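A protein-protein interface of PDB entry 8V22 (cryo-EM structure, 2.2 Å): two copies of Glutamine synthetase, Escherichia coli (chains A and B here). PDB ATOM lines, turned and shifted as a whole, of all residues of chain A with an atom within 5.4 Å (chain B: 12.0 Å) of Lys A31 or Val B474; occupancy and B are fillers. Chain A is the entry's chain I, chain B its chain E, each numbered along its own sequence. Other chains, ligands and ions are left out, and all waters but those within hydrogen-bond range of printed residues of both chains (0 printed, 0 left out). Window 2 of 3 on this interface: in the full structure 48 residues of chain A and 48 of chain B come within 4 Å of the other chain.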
ATOM      1  N   ASP A  29     -11.339   2.611 -14.690  1.00  0.00           N
ATOM      2  CA  ASP A  29     -10.655   1.630 -13.865  1.00  0.00           C
ATOM      3  C   ASP A  29     -11.441   0.320 -13.850  1.00  0.00           C
ATOM      4  O   ASP A  29     -12.484   0.181 -14.492  1.00  0.00           O
ATOM      5  CB  ASP A  29     -10.454   2.176 -12.455  1.00  0.00           C
ATOM      6  CG  ASP A  29     -11.762   2.446 -11.741  1.00  0.00           C
ATOM      7  OD1 ASP A  29     -12.819   2.439 -12.407  1.00  0.00           O
ATOM      8  OD2 ASP A  29     -11.732   2.672 -10.514  1.00  0.00           O
ATOM      9  N   THR A  30     -10.932  -0.659 -13.101  1.00  0.00           N
ATOM     10  CA  THR A  30     -11.562  -1.975 -13.085  1.00  0.00           C
ATOM     11  C   THR A  30     -12.985  -1.904 -12.549  1.00  0.00           C
ATOM     12  O   THR A  30     -13.894  -2.540 -13.095  1.00  0.00           O
ATOM     13  CB  THR A  30     -10.725  -2.945 -12.252  1.00  0.00           C
ATOM     14  OG1 THR A  30     -10.497  -2.388 -10.953  1.00  0.00           O
ATOM     15  CG2 THR A  30      -9.394  -3.209 -12.926  1.00  0.00           C
ATOM     16  N   LYS A  31     -13.200  -1.137 -11.481  1.00  0.00           N
ATOM     17  CA  LYS A  31     -14.534  -1.027 -10.907  1.00  0.00           C
ATOM     18  C   LYS A  31     -15.520  -0.346 -11.844  1.00  0.00           C
ATOM     19  O   LYS A  31     -16.730  -0.542 -11.694  1.00  0.00           O
ATOM     20  CB  LYS A  31     -14.473  -0.272  -9.582  1.00  0.00           C
ATOM     21  CG  LYS A  31     -13.769  -1.033  -8.479  1.00  0.00           C
ATOM     22  CD  LYS A  31     -13.793  -0.262  -7.177  1.00  0.00           C
ATOM     23  CE  LYS A  31     -12.997  -0.970  -6.100  1.00  0.00           C
ATOM     24  NZ  LYS A  31     -13.622  -2.267  -5.732  1.00  0.00           N
ATOM     25  N   GLY A  32     -15.040   0.445 -12.797  1.00  0.00           N
ATOM     26  CA  GLY A  32     -15.902   1.117 -13.744  1.00  0.00           C
ATOM     27  C   GLY A  32     -16.072   2.602 -13.517  1.00  0.00           C
ATOM     28  O   GLY A  32     -16.983   3.196 -14.105  1.00  0.00           O
ATOM     29  N   LYS A  33     -15.232   3.221 -12.695  1.00  0.00           N
ATOM     30  CA  LYS A  33     -15.326   4.642 -12.398  1.00  0.00           C
ATOM     31  C   LYS A  33     -14.374   5.422 -13.292  1.00  0.00           C
ATOM     32  O   LYS A  33     -13.231   5.008 -13.503  1.00  0.00           O
ATOM     33  CB  LYS A  33     -15.006   4.911 -10.926  1.00  0.00           C
ATOM     34  CG  LYS A  33     -15.274   6.340 -10.488  1.00  0.00           C
ATOM     35  CD  LYS A  33     -16.746   6.693 -10.579  1.00  0.00           C
ATOM     36  CE  LYS A  33     -17.019   8.071 -10.010  1.00  0.00           C
ATOM     37  NZ  LYS A  33     -18.445   8.462 -10.159  1.00  0.00           N
ATOM     38  N   PHE A 261     -26.653   5.086  -9.568  1.00  0.00           N
ATOM     39  CA  PHE A 261     -26.887   3.930 -10.420  1.00  0.00           C
ATOM     40  C   PHE A 261     -26.826   2.628  -9.631  1.00  0.00           C
ATOM     41  O   PHE A 261     -26.554   1.569 -10.204  1.00  0.00           O
ATOM     42  CB  PHE A 261     -25.874   3.917 -11.564  1.00  0.00           C
ATOM     43  CG  PHE A 261     -26.118   4.981 -12.591  1.00  0.00           C
ATOM     44  CD1 PHE A 261     -26.956   4.747 -13.665  1.00  0.00           C
ATOM     45  CD2 PHE A 261     -25.540   6.229 -12.461  1.00  0.00           C
ATOM     46  CE1 PHE A 261     -27.185   5.727 -14.605  1.00  0.00           C
ATOM     47  CE2 PHE A 261     -25.772   7.212 -13.396  1.00  0.00           C
ATOM     48  CZ  PHE A 261     -26.597   6.962 -14.466  1.00  0.00           C
ATOM     49  N   MET A 262     -27.068   2.688  -8.328  1.00  0.00           N
ATOM     50  CA  MET A 262     -27.067   1.479  -7.525  1.00  0.00           C
ATOM     51  C   MET A 262     -28.182   0.548  -7.992  1.00  0.00           C
ATOM     52  O   MET A 262     -29.271   1.015  -8.347  1.00  0.00           O
ATOM     53  CB  MET A 262     -27.268   1.810  -6.047  1.00  0.00           C
ATOM     54  CG  MET A 262     -25.989   1.983  -5.269  1.00  0.00           C
ATOM     55  SD  MET A 262     -26.315   2.181  -3.511  1.00  0.00           S
ATOM     56  CE  MET A 262     -27.217   3.722  -3.527  1.00  0.00           C
ATOM     57  N   PRO A 369     -26.782  -1.366 -13.795  1.00  0.00           N
ATOM     58  CA  PRO A 369     -25.952  -0.226 -14.213  1.00  0.00           C
ATOM     59  C   PRO A 369     -24.690  -0.038 -13.391  1.00  0.00           C
ATOM     60  O   PRO A 369     -23.838   0.768 -13.785  1.00  0.00           O
ATOM     61  CB  PRO A 369     -26.896   0.970 -14.061  1.00  0.00           C
ATOM     62  CG  PRO A 369     -27.897   0.549 -13.069  1.00  0.00           C
ATOM     63  CD  PRO A 369     -28.048  -0.932 -13.183  1.00  0.00           C
ATOM     64  N   ALA A 370     -24.535  -0.741 -12.269  1.00  0.00           N
ATOM     65  CA  ALA A 370     -23.293  -0.669 -11.513  1.00  0.00           C
ATOM     66  C   ALA A 370     -22.154  -1.416 -12.188  1.00  0.00           C
ATOM     67  O   ALA A 370     -21.009  -1.305 -11.737  1.00  0.00           O
ATOM     68  CB  ALA A 370     -23.502  -1.222 -10.104  1.00  0.00           C
ATOM     69  N   ALA A 371     -22.436  -2.172 -13.243  1.00  0.00           N
ATOM     70  CA  ALA A 371     -21.408  -2.954 -13.909  1.00  0.00           C
ATOM     71  C   ALA A 371     -20.438  -2.058 -14.666  1.00  0.00           C
ATOM     72  O   ALA A 371     -20.796  -0.983 -15.152  1.00  0.00           O
ATOM     73  CB  ALA A 371     -22.044  -3.949 -14.877  1.00  0.00           C
ATOM     74  N   ASN A 372     -19.197  -2.512 -14.761  1.00  0.00           N
ATOM     75  CA  ASN A 372     -18.244  -1.877 -15.656  1.00  0.00           C
ATOM     76  C   ASN A 372     -18.702  -2.145 -17.083  1.00  0.00           C
ATOM     77  O   ASN A 372     -18.812  -3.315 -17.474  1.00  0.00           O
ATOM     78  CB  ASN A 372     -16.841  -2.424 -15.425  1.00  0.00           C
ATOM     79  CG  ASN A 372     -15.785  -1.684 -16.217  1.00  0.00           C
ATOM     80  OD1 ASN A 372     -16.057  -1.143 -17.288  1.00  0.00           O
ATOM     81  ND2 ASN A 372     -14.566  -1.656 -15.693  1.00  0.00           N
ATOM     82  N   LEU A 451     -10.423  -7.671  -5.846  1.00  0.00           N
ATOM     83  CA  LEU A 451     -10.934  -6.328  -5.623  1.00  0.00           C
ATOM     84  C   LEU A 451     -12.403  -6.367  -5.226  1.00  0.00           C
ATOM     85  O   LEU A 451     -12.844  -5.587  -4.375  1.00  0.00           O
ATOM     86  CB  LEU A 451     -10.728  -5.492  -6.885  1.00  0.00           C
ATOM     87  CG  LEU A 451     -10.830  -3.976  -6.767  1.00  0.00           C
ATOM     88  CD1 LEU A 451      -9.742  -3.423  -5.860  1.00  0.00           C
ATOM     89  CD2 LEU A 451     -10.754  -3.347  -8.143  1.00  0.00           C
ATOM     90  N   ARG A 452     -13.178  -7.267  -5.835  1.00  0.00           N
ATOM     91  CA  ARG A 452     -14.582  -7.401  -5.457  1.00  0.00           C
ATOM     92  C   ARG A 452     -14.756  -8.153  -4.143  1.00  0.00           C
ATOM     93  O   ARG A 452     -15.688  -7.860  -3.380  1.00  0.00           O
ATOM     94  CB  ARG A 452     -15.357  -8.109  -6.568  1.00  0.00           C
ATOM     95  CG  ARG A 452     -15.471  -7.316  -7.859  1.00  0.00           C
ATOM     96  CD  ARG A 452     -15.976  -5.906  -7.618  1.00  0.00           C
ATOM     97  NE  ARG A 452     -16.383  -5.251  -8.853  1.00  0.00           N
ATOM     98  CZ  ARG A 452     -16.830  -4.005  -8.927  1.00  0.00           C
ATOM     99  NH1 ARG A 452     -16.935  -3.242  -7.851  1.00  0.00           N
ATOM    100  NH2 ARG A 452     -17.183  -3.513 -10.110  1.00  0.00           N
ATOM    101  N   GLU A 455     -14.788  -5.842  -1.030  1.00  0.00           N
ATOM    102  CA  GLU A 455     -16.083  -5.231  -0.755  1.00  0.00           C
ATOM    103  C   GLU A 455     -17.064  -6.255  -0.204  1.00  0.00           C
ATOM    104  O   GLU A 455     -17.832  -5.967   0.728  1.00  0.00           O
ATOM    105  CB  GLU A 455     -16.637  -4.608  -2.035  1.00  0.00           C
ATOM    106  CG  GLU A 455     -15.790  -3.488  -2.605  1.00  0.00           C
ATOM    107  CD  GLU A 455     -16.263  -3.045  -3.974  1.00  0.00           C
ATOM    108  OE1 GLU A 455     -17.031  -3.796  -4.613  1.00  0.00           O
ATOM    109  OE2 GLU A 455     -15.866  -1.946  -4.416  1.00  0.00           O
ATOM    110  N   PRO B 465     -26.165  -0.220   4.759  1.00  0.00           N
ATOM    111  CA  PRO B 465     -25.419   1.050   4.761  1.00  0.00           C
ATOM    112  C   PRO B 465     -23.996   0.922   4.253  1.00  0.00           C
ATOM    113  O   PRO B 465     -23.486   1.846   3.604  1.00  0.00           O
ATOM    114  CB  PRO B 465     -25.456   1.465   6.236  1.00  0.00           C
ATOM    115  CG  PRO B 465     -26.679   0.844   6.771  1.00  0.00           C
ATOM    116  CD  PRO B 465     -26.881  -0.436   6.027  1.00  0.00           C
ATOM    117  N   VAL B 466     -23.323  -0.191   4.544  1.00  0.00           N
ATOM    118  CA  VAL B 466     -22.009  -0.425   3.960  1.00  0.00           C
ATOM    119  C   VAL B 466     -22.121  -0.538   2.449  1.00  0.00           C
ATOM    120  O   VAL B 466     -21.231  -0.087   1.715  1.00  0.00           O
ATOM    121  CB  VAL B 466     -21.362  -1.676   4.585  1.00  0.00           C
ATOM    122  CG1 VAL B 466     -20.140  -2.111   3.801  1.00  0.00           C
ATOM    123  CG2 VAL B 466     -20.977  -1.394   6.020  1.00  0.00           C
ATOM    124  N   GLU B 467     -23.212  -1.125   1.954  1.00  0.00           N
ATOM    125  CA  GLU B 467     -23.416  -1.159   0.512  1.00  0.00           C
ATOM    126  C   GLU B 467     -23.541   0.241  -0.064  1.00  0.00           C
ATOM    127  O   GLU B 467     -23.009   0.509  -1.144  1.00  0.00           O
ATOM    128  CB  GLU B 467     -24.650  -1.984   0.153  1.00  0.00           C
ATOM    129  CG  GLU B 467     -24.442  -3.468   0.282  1.00  0.00           C
ATOM    130  CD  GLU B 467     -25.691  -4.254  -0.028  1.00  0.00           C
ATOM    131  OE1 GLU B 467     -26.789  -3.660  -0.019  1.00  0.00           O
ATOM    132  OE2 GLU B 467     -25.572  -5.465  -0.302  1.00  0.00           O
ATOM    133  N   PHE B 468     -24.228   1.149   0.629  1.00  0.00           N
ATOM    134  CA  PHE B 468     -24.231   2.529   0.146  1.00  0.00           C
ATOM    135  C   PHE B 468     -22.832   3.129   0.177  1.00  0.00           C
ATOM    136  O   PHE B 468     -22.386   3.720  -0.814  1.00  0.00           O
ATOM    137  CB  PHE B 468     -25.196   3.388   0.957  1.00  0.00           C
ATOM    138  CG  PHE B 468     -26.640   3.077   0.705  1.00  0.00           C
ATOM    139  CD1 PHE B 468     -27.225   1.940   1.220  1.00  0.00           C
ATOM    140  CD2 PHE B 468     -27.415   3.939  -0.044  1.00  0.00           C
ATOM    141  CE1 PHE B 468     -28.549   1.664   0.983  1.00  0.00           C
ATOM    142  CE2 PHE B 468     -28.738   3.667  -0.284  1.00  0.00           C
ATOM    143  CZ  PHE B 468     -29.306   2.528   0.232  1.00  0.00           C
ATOM    144  N   GLU B 469     -22.107   2.936   1.281  1.00  0.00           N
ATOM    145  CA  GLU B 469     -20.761   3.492   1.388  1.00  0.00           C
ATOM    146  C   GLU B 469     -19.872   3.009   0.255  1.00  0.00           C
ATOM    147  O   GLU B 469     -18.977   3.736  -0.189  1.00  0.00           O
ATOM    148  CB  GLU B 469     -20.127   3.109   2.725  1.00  0.00           C
ATOM    149  CG  GLU B 469     -20.747   3.774   3.931  1.00  0.00           C
ATOM    150  CD  GLU B 469     -20.078   3.355   5.222  1.00  0.00           C
ATOM    151  OE1 GLU B 469     -19.230   2.437   5.182  1.00  0.00           O
ATOM    152  OE2 GLU B 469     -20.402   3.932   6.281  1.00  0.00           O
ATOM    153  N   LEU B 470     -20.102   1.791  -0.225  1.00  0.00           N
ATOM    154  CA  LEU B 470     -19.236   1.197  -1.232  1.00  0.00           C
ATOM    155  C   LEU B 470     -19.682   1.506  -2.655  1.00  0.00           C
ATOM    156  O   LEU B 470     -18.838   1.714  -3.531  1.00  0.00           O
ATOM    157  CB  LEU B 470     -19.182  -0.320  -1.047  1.00  0.00           C
ATOM    158  CG  LEU B 470     -18.312  -0.830   0.101  1.00  0.00           C
ATOM    159  CD1 LEU B 470     -18.659  -2.275   0.412  1.00  0.00           C
ATOM    160  CD2 LEU B 470     -16.832  -0.678  -0.209  1.00  0.00           C
ATOM    161  N   TYR B 471     -20.990   1.543  -2.908  1.00  0.00           N
ATOM    162  CA  TYR B 471     -21.508   1.533  -4.265  1.00  0.00           C
ATOM    163  C   TYR B 471     -22.355   2.742  -4.633  1.00  0.00           C
ATOM    164  O   TYR B 471     -22.882   2.776  -5.749  1.00  0.00           O
ATOM    165  CB  TYR B 471     -22.354   0.274  -4.492  1.00  0.00           C
ATOM    166  CG  TYR B 471     -21.652  -1.017  -4.162  1.00  0.00           C
ATOM    167  CD1 TYR B 471     -20.445  -1.345  -4.753  1.00  0.00           C
ATOM    168  CD2 TYR B 471     -22.208  -1.916  -3.268  1.00  0.00           C
ATOM    169  CE1 TYR B 471     -19.805  -2.526  -4.455  1.00  0.00           C
ATOM    170  CE2 TYR B 471     -21.578  -3.098  -2.964  1.00  0.00           C
ATOM    171  CZ  TYR B 471     -20.378  -3.400  -3.560  1.00  0.00           C
ATOM    172  OH  TYR B 471     -19.745  -4.581  -3.260  1.00  0.00           O
ATOM    173  N   TYR B 472     -22.517   3.729  -3.751  1.00  0.00           N
ATOM    174  CA  TYR B 472     -23.397   4.839  -4.101  1.00  0.00           C
ATOM    175  C   TYR B 472     -22.887   5.583  -5.325  1.00  0.00           C
ATOM    176  O   TYR B 472     -23.674   5.984  -6.190  1.00  0.00           O
ATOM    177  CB  TYR B 472     -23.561   5.799  -2.930  1.00  0.00           C
ATOM    178  CG  TYR B 472     -24.572   6.879  -3.229  1.00  0.00           C
ATOM    179  CD1 TYR B 472     -25.926   6.648  -3.067  1.00  0.00           C
ATOM    180  CD2 TYR B 472     -24.172   8.121  -3.695  1.00  0.00           C
ATOM    181  CE1 TYR B 472     -26.852   7.624  -3.350  1.00  0.00           C
ATOM    182  CE2 TYR B 472     -25.092   9.102  -3.978  1.00  0.00           C
ATOM    183  CZ  TYR B 472     -26.428   8.850  -3.807  1.00  0.00           C
ATOM    184  OH  TYR B 472     -27.347   9.831  -4.089  1.00  0.00           O
ATOM    185  N   SER B 473     -21.577   5.788  -5.416  1.00  0.00           N
ATOM    186  CA  SER B 473     -20.981   6.504  -6.532  1.00  0.00           C
ATOM    187  C   SER B 473     -20.627   5.597  -7.701  1.00  0.00           C
ATOM    188  O   SER B 473     -20.097   6.086  -8.702  1.00  0.00           O
ATOM    189  CB  SER B 473     -19.728   7.246  -6.067  1.00  0.00           C
ATOM    190  OG  SER B 473     -20.027   8.132  -5.004  1.00  0.00           O
ATOM    191  N   VAL B 474     -20.894   4.299  -7.601  1.00  0.00           N
ATOM    192  CA  VAL B 474     -20.586   3.367  -8.677  1.00  0.00           C
ATOM    193  C   VAL B 474     -21.755   2.417  -8.879  1.00  0.00           C
ATOM    194  O   VAL B 474     -22.829   2.825  -9.316  1.00  0.00           O
ATOM    195  CB  VAL B 474     -19.291   2.581  -8.386  1.00  0.00           C
ATOM    196  CG1 VAL B 474     -18.981   1.614  -9.524  1.00  0.00           C
ATOM    197  CG2 VAL B 474     -18.126   3.534  -8.154  1.00  0.00           C
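Of the 14 printed residues of chain A, 5 touch a printed residue of chain B.
Hydrophobic or aromatic side chains of chain A that line the printed part of chain B: Phe A261 and Met A262.
Hydrophobic or aromatic side chains of chain B within 4 Å of the printed part of chain A: Phe B468, Leu B470, Tyr B471, Tyr B472 and Val B474.
Among the printed residues, 8 pairs touch across the chains.
Among the printed residues, no Asp or Glu carboxylate lies within 4 Å of a Lys or Arg side-chain nitrogen of the other chain.
Among the printed residues, merely in contact across the chains: Lys A31 with Val B474, Phe A261 with Val B474, Met A262 with Phe B468, Met A262 with Tyr B471, Met A262 with Tyr B472 and Glu A455 with Leu B470.
No residue of chain B comes within 4 Å of Asp A29.
No residue of chain B comes within 4 Å of Thr A30.
No residue of chain B comes within 4 Å of Gly A32.
Of chain B, only Ser B473 comes within 4 Å of Lys A33.
Phe A261 touches one residue of chain B.
No residue of chain B comes within 4 Å of Pro A369.
No residue of chain B comes within 4 Å of Ala A371.
No residue of chain B comes within 4 Å of Asn A372.
Pro B465 touches none of the printed residues of chain A.
Glu B467 touches none of the printed residues of chain A.
Of the printed residues of chain A, Phe B468 touches Met A262 (3.5 Å).
Printed residues of chain A within 4 Å of Tyr B472: Met A262 (3.2 Å).
Printed residues of chain A within 4 Å of Val B474: Lys A31 (3.8 Å) and Phe A261 (3.9 Å).
The nearest residue of chain B that does not touch Lys A31 is Tyr B471 (6.3 Å).
NZ of Lys A33 sits at hydrogen-bond distance from O of Ser B473 (3.2 Å).
OE1 of Glu A455 sits close to OH of Tyr B471, 3.1 Å away.
No position is printed for both chains.
Of the 8 pairs that touch across the chains among the printed residues, none has its exchanged pair printed and touching as well.
OD1 of Asp A29 lies within hydrogen-bond range of N of Lys A33 (2.6 Å).
NH1 of Arg A452 is in salt-bridge range of OE1 of Glu A455 (3.3 Å).
The side-chain carboxylate (OE2) of Glu A455 is in salt-bridge range of the side-chain amino group (NZ) of Lys A31, 2.6 Å away.
NH2 of Arg A452 is in hydrogen-bond range of O of Lys A31, 3.4 Å away.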
